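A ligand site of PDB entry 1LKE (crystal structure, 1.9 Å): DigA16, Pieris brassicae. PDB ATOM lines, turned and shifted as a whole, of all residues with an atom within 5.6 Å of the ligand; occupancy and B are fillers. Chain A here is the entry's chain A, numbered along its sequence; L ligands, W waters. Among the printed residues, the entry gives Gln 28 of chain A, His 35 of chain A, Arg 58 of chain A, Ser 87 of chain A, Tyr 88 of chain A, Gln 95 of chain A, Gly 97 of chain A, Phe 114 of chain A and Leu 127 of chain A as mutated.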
ATOM      1  N   TRP A  26      14.225   9.387  18.700  1.00  0.00           N
ATOM      2  CA  TRP A  26      13.290   9.687  17.621  1.00  0.00           C
ATOM      3  C   TRP A  26      13.534   8.752  16.439  1.00  0.00           C
ATOM      4  O   TRP A  26      14.677   8.588  16.018  1.00  0.00           O
ATOM      5  CB  TRP A  26      13.495  11.119  17.141  1.00  0.00           C
ATOM      6  CG  TRP A  26      13.064  12.125  18.164  1.00  0.00           C
ATOM      7  CD1 TRP A  26      13.756  12.510  19.291  1.00  0.00           C
ATOM      8  CD2 TRP A  26      11.841  12.859  18.193  1.00  0.00           C
ATOM      9  NE1 TRP A  26      13.038  13.448  19.988  1.00  0.00           N
ATOM     10  CE2 TRP A  26      11.857  13.681  19.345  1.00  0.00           C
ATOM     11  CE3 TRP A  26      10.704  12.901  17.373  1.00  0.00           C
ATOM     12  CZ2 TRP A  26      10.814  14.519  19.657  1.00  0.00           C
ATOM     13  CZ3 TRP A  26       9.676  13.735  17.700  1.00  0.00           C
ATOM     14  CH2 TRP A  26       9.746  14.555  18.829  1.00  0.00           C
ATOM     15  N   GLN A  28      13.033   7.633  12.471  1.00  0.00           N
ATOM     16  CA  GLN A  28      12.756   8.244  11.199  1.00  0.00           C
ATOM     17  C   GLN A  28      11.744   7.386  10.377  1.00  0.00           C
ATOM     18  O   GLN A  28      12.153   6.515   9.590  1.00  0.00           O
ATOM     19  CB  GLN A  28      14.039   8.426  10.418  1.00  0.00           C
ATOM     20  CG  GLN A  28      13.856   9.294   9.186  1.00  0.00           C
ATOM     21  CD  GLN A  28      15.140   9.450   8.437  1.00  0.00           C
ATOM     22  OE1 GLN A  28      16.147   9.977   9.001  1.00  0.00           O
ATOM     23  NE2 GLN A  28      15.167   8.962   7.210  1.00  0.00           N
ATOM     24  N   HIS A  35      16.778  10.908   0.204  1.00  0.00           N
ATOM     25  CA  HIS A  35      17.242  11.023   1.613  1.00  0.00           C
ATOM     26  C   HIS A  35      17.627   9.639   2.195  1.00  0.00           C
ATOM     27  O   HIS A  35      18.670   9.464   2.878  1.00  0.00           O
ATOM     28  CB  HIS A  35      16.146  11.664   2.458  1.00  0.00           C
ATOM     29  CG  HIS A  35      16.604  12.083   3.828  1.00  0.00           C
ATOM     30  ND1 HIS A  35      16.732  11.199   4.871  1.00  0.00           N
ATOM     31  CD2 HIS A  35      16.965  13.296   4.307  1.00  0.00           C
ATOM     32  CE1 HIS A  35      17.147  11.850   5.952  1.00  0.00           C
ATOM     33  NE2 HIS A  35      17.271  13.120   5.646  1.00  0.00           N
ATOM     34  N   TYR A  39      21.361   9.155   3.291  1.00  0.00           N
ATOM     35  CA  TYR A  39      21.556   9.203   4.748  1.00  0.00           C
ATOM     36  C   TYR A  39      21.177   7.946   5.423  1.00  0.00           C
ATOM     37  O   TYR A  39      21.351   7.805   6.627  1.00  0.00           O
ATOM     38  CB  TYR A  39      20.825  10.446   5.361  1.00  0.00           C
ATOM     39  CG  TYR A  39      21.307  11.685   4.667  1.00  0.00           C
ATOM     40  CD1 TYR A  39      20.499  12.362   3.727  1.00  0.00           C
ATOM     41  CD2 TYR A  39      22.598  12.154   4.885  1.00  0.00           C
ATOM     42  CE1 TYR A  39      20.956  13.469   3.061  1.00  0.00           C
ATOM     43  CE2 TYR A  39      23.081  13.274   4.196  1.00  0.00           C
ATOM     44  CZ  TYR A  39      22.261  13.913   3.303  1.00  0.00           C
ATOM     45  OH  TYR A  39      22.717  15.001   2.613  1.00  0.00           O
ATOM     46  N   ALA A  45      17.595   8.273  15.956  1.00  0.00           N
ATOM     47  CA  ALA A  45      18.625   9.122  16.554  1.00  0.00           C
ATOM     48  C   ALA A  45      18.305   9.386  18.012  1.00  0.00           C
ATOM     49  O   ALA A  45      17.152   9.419  18.386  1.00  0.00           O
ATOM     50  CB  ALA A  45      18.709  10.380  15.829  1.00  0.00           C
ATOM     51  N   TYR A  47      18.829  12.160  21.037  1.00  0.00           N
ATOM     52  CA  TYR A  47      19.148  13.581  21.225  1.00  0.00           C
ATOM     53  C   TYR A  47      19.456  13.806  22.694  1.00  0.00           C
ATOM     54  O   TYR A  47      18.647  13.504  23.549  1.00  0.00           O
ATOM     55  CB  TYR A  47      17.937  14.438  20.833  1.00  0.00           C
ATOM     56  CG  TYR A  47      17.720  14.510  19.334  1.00  0.00           C
ATOM     57  CD1 TYR A  47      17.155  13.447  18.650  1.00  0.00           C
ATOM     58  CD2 TYR A  47      18.147  15.602  18.603  1.00  0.00           C
ATOM     59  CE1 TYR A  47      16.964  13.500  17.249  1.00  0.00           C
ATOM     60  CE2 TYR A  47      17.960  15.663  17.200  1.00  0.00           C
ATOM     61  CZ  TYR A  47      17.355  14.607  16.540  1.00  0.00           C
ATOM     62  OH  TYR A  47      17.185  14.640  15.151  1.00  0.00           O
ATOM     63  N   VAL A  56      23.558  14.976  18.921  1.00  0.00           N
ATOM     64  CA  VAL A  56      22.783  14.047  18.124  1.00  0.00           C
ATOM     65  C   VAL A  56      23.622  12.831  17.792  1.00  0.00           C
ATOM     66  O   VAL A  56      24.662  12.966  17.176  1.00  0.00           O
ATOM     67  CB  VAL A  56      22.384  14.676  16.758  1.00  0.00           C
ATOM     68  CG1 VAL A  56      21.471  13.736  15.976  1.00  0.00           C
ATOM     69  CG2 VAL A  56      21.782  16.053  16.932  1.00  0.00           C
ATOM     70  N   ARG A  58      23.325   9.267  15.723  1.00  0.00           N
ATOM     71  CA  ARG A  58      22.305   8.722  14.815  1.00  0.00           C
ATOM     72  C   ARG A  58      22.785   7.425  14.215  1.00  0.00           C
ATOM     73  O   ARG A  58      23.953   7.319  13.830  1.00  0.00           O
ATOM     74  CB  ARG A  58      22.061   9.701  13.669  1.00  0.00           C
ATOM     75  CG  ARG A  58      21.004   9.261  12.646  1.00  0.00           C
ATOM     76  CD  ARG A  58      20.730  10.372  11.594  1.00  0.00           C
ATOM     77  NE  ARG A  58      19.704   9.987  10.651  1.00  0.00           N
ATOM     78  CZ  ARG A  58      19.958   9.486   9.456  1.00  0.00           C
ATOM     79  NH1 ARG A  58      21.210   9.308   9.037  1.00  0.00           N
ATOM     80  NH2 ARG A  58      18.955   9.203   8.650  1.00  0.00           N
ATOM     81  N   HIS A  86      22.377  21.905  12.216  1.00  0.00           N
ATOM     82  CA  HIS A  86      22.994  20.668  12.666  1.00  0.00           C
ATOM     83  C   HIS A  86      24.328  20.540  12.022  1.00  0.00           C
ATOM     84  O   HIS A  86      24.475  20.857  10.831  1.00  0.00           O
ATOM     85  CB  HIS A  86      22.233  19.432  12.174  1.00  0.00           C
ATOM     86  CG  HIS A  86      21.121  18.981  13.062  1.00  0.00           C
ATOM     87  ND1 HIS A  86      20.566  17.728  12.972  1.00  0.00           N
ATOM     88  CD2 HIS A  86      20.383  19.654  13.985  1.00  0.00           C
ATOM     89  CE1 HIS A  86      19.569  17.619  13.826  1.00  0.00           C
ATOM     90  NE2 HIS A  86      19.413  18.786  14.423  1.00  0.00           N
ATOM     91  N   SER A  87      25.305  20.027  12.769  1.00  0.00           N
ATOM     92  CA  SER A  87      26.515  19.566  12.099  1.00  0.00           C
ATOM     93  C   SER A  87      26.259  18.064  11.921  1.00  0.00           C
ATOM     94  O   SER A  87      25.413  17.501  12.604  1.00  0.00           O
ATOM     95  CB  SER A  87      27.783  19.787  12.930  1.00  0.00           C
ATOM     96  OG  SER A  87      27.679  19.117  14.186  1.00  0.00           O
ATOM     97  N   TYR A  88      27.034  17.405  11.074  1.00  0.00           N
ATOM     98  CA  TYR A  88      26.749  15.986  10.727  1.00  0.00           C
ATOM     99  C   TYR A  88      28.114  15.359  10.348  1.00  0.00           C
ATOM    100  O   TYR A  88      28.657  15.680   9.288  1.00  0.00           O
ATOM    101  CB  TYR A  88      25.828  15.955   9.502  1.00  0.00           C
ATOM    102  CG  TYR A  88      25.505  14.585   8.974  1.00  0.00           C
ATOM    103  CD1 TYR A  88      24.685  13.727   9.684  1.00  0.00           C
ATOM    104  CD2 TYR A  88      26.031  14.162   7.770  1.00  0.00           C
ATOM    105  CE1 TYR A  88      24.390  12.446   9.223  1.00  0.00           C
ATOM    106  CE2 TYR A  88      25.751  12.861   7.275  1.00  0.00           C
ATOM    107  CZ  TYR A  88      24.932  12.018   8.034  1.00  0.00           C
ATOM    108  OH  TYR A  88      24.640  10.769   7.604  1.00  0.00           O
ATOM    109  N   GLN A  95      29.945  17.752   7.858  1.00  0.00           N
ATOM    110  CA  GLN A  95      29.200  18.684   7.043  1.00  0.00           C
ATOM    111  C   GLN A  95      28.316  19.489   7.997  1.00  0.00           C
ATOM    112  O   GLN A  95      28.118  19.078   9.141  1.00  0.00           O
ATOM    113  CB  GLN A  95      28.304  17.923   6.058  1.00  0.00           C
ATOM    114  CG  GLN A  95      29.060  17.192   4.910  1.00  0.00           C
ATOM    115  CD  GLN A  95      28.139  16.226   4.181  1.00  0.00           C
ATOM    116  OE1 GLN A  95      27.327  16.645   3.402  1.00  0.00           O
ATOM    117  NE2 GLN A  95      28.266  14.937   4.472  1.00  0.00           N
ATOM    118  N   GLU A  96      27.785  20.617   7.552  1.00  0.00           N
ATOM    119  CA  GLU A  96      26.866  21.349   8.443  1.00  0.00           C
ATOM    120  C   GLU A  96      25.826  22.048   7.598  1.00  0.00           C
ATOM    121  O   GLU A  96      26.044  22.280   6.422  1.00  0.00           O
ATOM    122  CB  GLU A  96      27.617  22.343   9.329  1.00  0.00           C
ATOM    123  CG  GLU A  96      28.410  23.411   8.549  1.00  0.00           C
ATOM    124  CD  GLU A  96      29.268  24.302   9.419  1.00  0.00           C
ATOM    125  OE1 GLU A  96      29.940  25.214   8.837  1.00  0.00           O
ATOM    126  OE2 GLU A  96      29.296  24.128  10.667  1.00  0.00           O
ATOM    127  N   GLY A  97      24.696  22.402   8.194  1.00  0.00           N
ATOM    128  CA  GLY A  97      23.698  23.099   7.422  1.00  0.00           C
ATOM    129  C   GLY A  97      22.527  23.510   8.273  1.00  0.00           C
ATOM    130  O   GLY A  97      22.426  23.120   9.435  1.00  0.00           O
ATOM    131  N   VAL A  98      21.600  24.248   7.649  1.00  0.00           N
ATOM    132  CA  VAL A  98      20.411  24.708   8.355  1.00  0.00           C
ATOM    133  C   VAL A  98      19.187  24.124   7.670  1.00  0.00           C
ATOM    134  O   VAL A  98      19.124  24.128   6.465  1.00  0.00           O
ATOM    135  CB  VAL A  98      20.300  26.257   8.387  1.00  0.00           C
ATOM    136  CG1 VAL A  98      19.023  26.691   9.111  1.00  0.00           C
ATOM    137  CG2 VAL A  98      21.500  26.865   9.102  1.00  0.00           C
ATOM    138  N   PHE A  99      18.263  23.586   8.439  1.00  0.00           N
ATOM    139  CA  PHE A  99      17.021  23.052   7.840  1.00  0.00           C
ATOM    140  C   PHE A  99      15.837  23.703   8.556  1.00  0.00           C
ATOM    141  O   PHE A  99      15.998  24.368   9.589  1.00  0.00           O
ATOM    142  CB  PHE A  99      16.964  21.529   7.890  1.00  0.00           C
ATOM    143  CG  PHE A  99      16.775  20.972   9.271  1.00  0.00           C
ATOM    144  CD1 PHE A  99      15.530  20.634   9.739  1.00  0.00           C
ATOM    145  CD2 PHE A  99      17.869  20.629  10.011  1.00  0.00           C
ATOM    146  CE1 PHE A  99      15.322  20.099  11.042  1.00  0.00           C
ATOM    147  CE2 PHE A  99      17.715  20.087  11.315  1.00  0.00           C
ATOM    148  CZ  PHE A  99      16.428  19.828  11.842  1.00  0.00           C
ATOM    149  N   PHE A 114      14.785  20.359   3.741  1.00  0.00           N
ATOM    150  CA  PHE A 114      16.008  21.018   3.333  1.00  0.00           C
ATOM    151  C   PHE A 114      15.928  21.174   1.821  1.00  0.00           C
ATOM    152  O   PHE A 114      15.524  20.282   1.137  1.00  0.00           O
ATOM    153  CB  PHE A 114      17.190  20.117   3.683  1.00  0.00           C
ATOM    154  CG  PHE A 114      18.515  20.688   3.263  1.00  0.00           C
ATOM    155  CD1 PHE A 114      19.120  20.244   2.102  1.00  0.00           C
ATOM    156  CD2 PHE A 114      19.097  21.712   4.010  1.00  0.00           C
ATOM    157  CE1 PHE A 114      20.331  20.777   1.690  1.00  0.00           C
ATOM    158  CE2 PHE A 114      20.315  22.244   3.610  1.00  0.00           C
ATOM    159  CZ  PHE A 114      20.939  21.769   2.421  1.00  0.00           C
ATOM    160  N   LEU A 127      14.586  17.634   0.104  1.00  0.00           N
ATOM    161  CA  LEU A 127      14.659  16.457   0.953  1.00  0.00           C
ATOM    162  C   LEU A 127      13.737  16.683   2.096  1.00  0.00           C
ATOM    163  O   LEU A 127      13.765  17.738   2.716  1.00  0.00           O
ATOM    164  CB  LEU A 127      16.047  16.323   1.568  1.00  0.00           C
ATOM    165  CG  LEU A 127      17.162  15.985   0.580  1.00  0.00           C
ATOM    166  CD1 LEU A 127      18.512  16.245   1.233  1.00  0.00           C
ATOM    167  CD2 LEU A 127      17.072  14.489   0.044  1.00  0.00           C
ATOM    168  N   TRP A 129      12.053  14.598   5.643  1.00  0.00           N
ATOM    169  CA  TRP A 129      12.096  13.460   6.526  1.00  0.00           C
ATOM    170  C   TRP A 129      11.145  13.685   7.686  1.00  0.00           C
ATOM    171  O   TRP A 129      10.938  14.820   8.124  1.00  0.00           O
ATOM    172  CB  TRP A 129      13.547  13.188   7.044  1.00  0.00           C
ATOM    173  CG  TRP A 129      14.170  14.313   7.843  1.00  0.00           C
ATOM    174  CD1 TRP A 129      14.205  14.446   9.240  1.00  0.00           C
ATOM    175  CD2 TRP A 129      14.842  15.473   7.323  1.00  0.00           C
ATOM    176  NE1 TRP A 129      14.853  15.615   9.576  1.00  0.00           N
ATOM    177  CE2 TRP A 129      15.283  16.250   8.433  1.00  0.00           C
ATOM    178  CE3 TRP A 129      15.179  15.907   6.018  1.00  0.00           C
ATOM    179  CZ2 TRP A 129      16.010  17.432   8.274  1.00  0.00           C
ATOM    180  CZ3 TRP A 129      15.874  17.097   5.861  1.00  0.00           C
ATOM    181  CH2 TRP A 129      16.275  17.857   6.993  1.00  0.00           C
ATOM    182  N   LEU A 131      10.119  12.505  11.550  1.00  0.00           N
ATOM    183  CA  LEU A 131      10.566  11.878  12.781  1.00  0.00           C
ATOM    184  C   LEU A 131       9.377  11.665  13.711  1.00  0.00           C
ATOM    185  O   LEU A 131       8.506  12.497  13.791  1.00  0.00           O
ATOM    186  CB  LEU A 131      11.562  12.795  13.531  1.00  0.00           C
ATOM    187  CG  LEU A 131      12.907  13.141  12.890  1.00  0.00           C
ATOM    188  CD1 LEU A 131      13.831  13.761  13.937  1.00  0.00           C
ATOM    189  CD2 LEU A 131      13.545  11.909  12.257  1.00  0.00           C
HETATM  190  O1  LIG L   1      17.066  12.740  13.399  1.00  0.00           O
HETATM  191  C1  LIG L   1      17.528  12.920  12.317  1.00  0.00           C
HETATM  192  C2  LIG L   1      18.836  13.400  11.954  1.00  0.00           C
HETATM  193  O2  LIG L   1      16.855  12.663  11.173  1.00  0.00           O
HETATM  194  C3  LIG L   1      17.674  12.921  10.009  1.00  0.00           C
HETATM  195  C4  LIG L   1      18.929  13.414  10.617  1.00  0.00           C
HETATM  196  C5  LIG L   1      20.046  13.849   9.759  1.00  0.00           C
HETATM  197  C6  LIG L   1      20.252  13.069   8.430  1.00  0.00           C
HETATM  198  C7  LIG L   1      20.029  15.385   9.351  1.00  0.00           C
HETATM  199  C8  LIG L   1      19.021  16.226  10.117  1.00  0.00           C
HETATM  200  C9  LIG L   1      21.460  15.925   9.597  1.00  0.00           C
HETATM  201  O3  LIG L   1      21.699  16.068  11.022  1.00  0.00           O
HETATM  202  C10 LIG L   1      19.756  15.359   7.817  1.00  0.00           C
HETATM  203  C11 LIG L   1      20.528  14.112   7.344  1.00  0.00           C
HETATM  204  O4  LIG L   1      18.370  15.003   7.591  1.00  0.00           O
HETATM  205  C12 LIG L   1      20.113  16.666   7.107  1.00  0.00           C
HETATM  206  C13 LIG L   1      19.985  16.535   5.585  1.00  0.00           C
HETATM  207  C14 LIG L   1      21.512  17.247   7.461  1.00  0.00           C
HETATM  208  C15 LIG L   1      21.699  17.283   9.021  1.00  0.00           C
HETATM  209  C16 LIG L   1      21.727  18.624   6.786  1.00  0.00           C
HETATM  210  C17 LIG L   1      20.723  19.685   7.308  1.00  0.00           C
HETATM  211  C18 LIG L   1      21.594  18.486   5.233  1.00  0.00           C
HETATM  212  C19 LIG L   1      20.256  17.834   4.842  1.00  0.00           C
HETATM  213  C20 LIG L   1      22.734  17.659   4.604  1.00  0.00           C
HETATM  214  C21 LIG L   1      24.113  18.206   5.002  1.00  0.00           C
HETATM  215  O5  LIG L   1      24.283  19.463   4.358  1.00  0.00           O
HETATM  216  C22 LIG L   1      24.261  18.326   6.488  1.00  0.00           C
HETATM  217  C23 LIG L   1      23.146  19.170   7.070  1.00  0.00           C
HETATM  218  O   HOH W   1      23.583  15.313  12.710  1.00  0.00           O
HETATM  219  O   HOH W   2      15.814  10.096  13.888  1.00  0.00           O
HETATM  220  O   HOH W   3      17.119   9.605  11.626  1.00  0.00           O
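An oxygen (O4) of the ligand lies within hydrogen-bond range of a ring nitrogen (NE2) of His 35, 2.9 Å away. An oxygen (O1) of the ligand sits at hydrogen-bond distance from the side-chain hydroxyl (OH) of Tyr 47, at 2.6 Å. ND1 of His 86 sits at hydrogen-bond distance from O3 of the ligand (2.8 Å).
The backbone carbonyl oxygen of Gly 97 is in hydrogen-bond range of the backbone NH of His 86. The backbone NH (N) of Ala 45 sits at hydrogen-bond distance from the backbone carbonyl oxygen (O) of Trp 26 (2.9 Å). The backbone carbonyl oxygen (O) of Phe 114 sits at hydrogen-bond distance from the backbone NH (N) of Leu 127, 3.0 Å away. N of Tyr 88 lies within hydrogen-bond range of O of Gln 95 (2.8 Å). NH1 of Arg 58 sits at hydrogen-bond distance from O of Tyr 39 (2.8 Å). The side-chain amide oxygen (OE1) of Gln 28 lies within hydrogen-bond range of the guanidinium group (NH2) of Arg 58 (2.9 Å).
Merely in contact with the ligand: Tyr 39 (3.3 Å), Trp 129 (3.4 Å), Leu 131 (3.4 Å), Gln 28 (3.5 Å), Arg 58 (3.5 Å), Phe 114 (3.7 Å), Gly 97 (3.8 Å), Ala 45 (3.8 Å), Tyr 88 (3.9 Å), Glu 96 (3.9 Å) and Gln 95 (3.9 Å). Hydrophobic or aromatic side chains within 4 Å of the ligand: His 35, Tyr 39, Ala 45, Tyr 47, His 86, Tyr 88, Phe 114, Trp 129 and Leu 131. Within 4 Å of the ligand: Gln 28, His 35, Tyr 39, Ala 45, Tyr 47, Arg 58, His 86, Tyr 88, Gln 95, Glu 96, Gly 97, Phe 114, Trp 129 and Leu 131. Along chain A the residues within 4 Å of the ligand span positions 28 to 131. The nearest printed residue that does not touch the ligand is Phe 99 (4.04 Å).
Water W1 lies within hydrogen-bond range of an oxygen (O3) of the ligand (2.6 Å) and the backbone carbonyl oxygen (O) of Ser 87 (2.9 Å). Water W2 lies within hydrogen-bond range of O of Trp 26 (2.8 Å), O1 of the ligand (3.0 Å) and N of Ala 45 (3.3 Å). Water W3 lies within hydrogen-bond range of the guanidinium group of Arg 58 (2.8 Å), the side-chain amide oxygen of Gln 28 (2.8 Å) and an oxygen (O2) of the ligand (3.1 Å).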
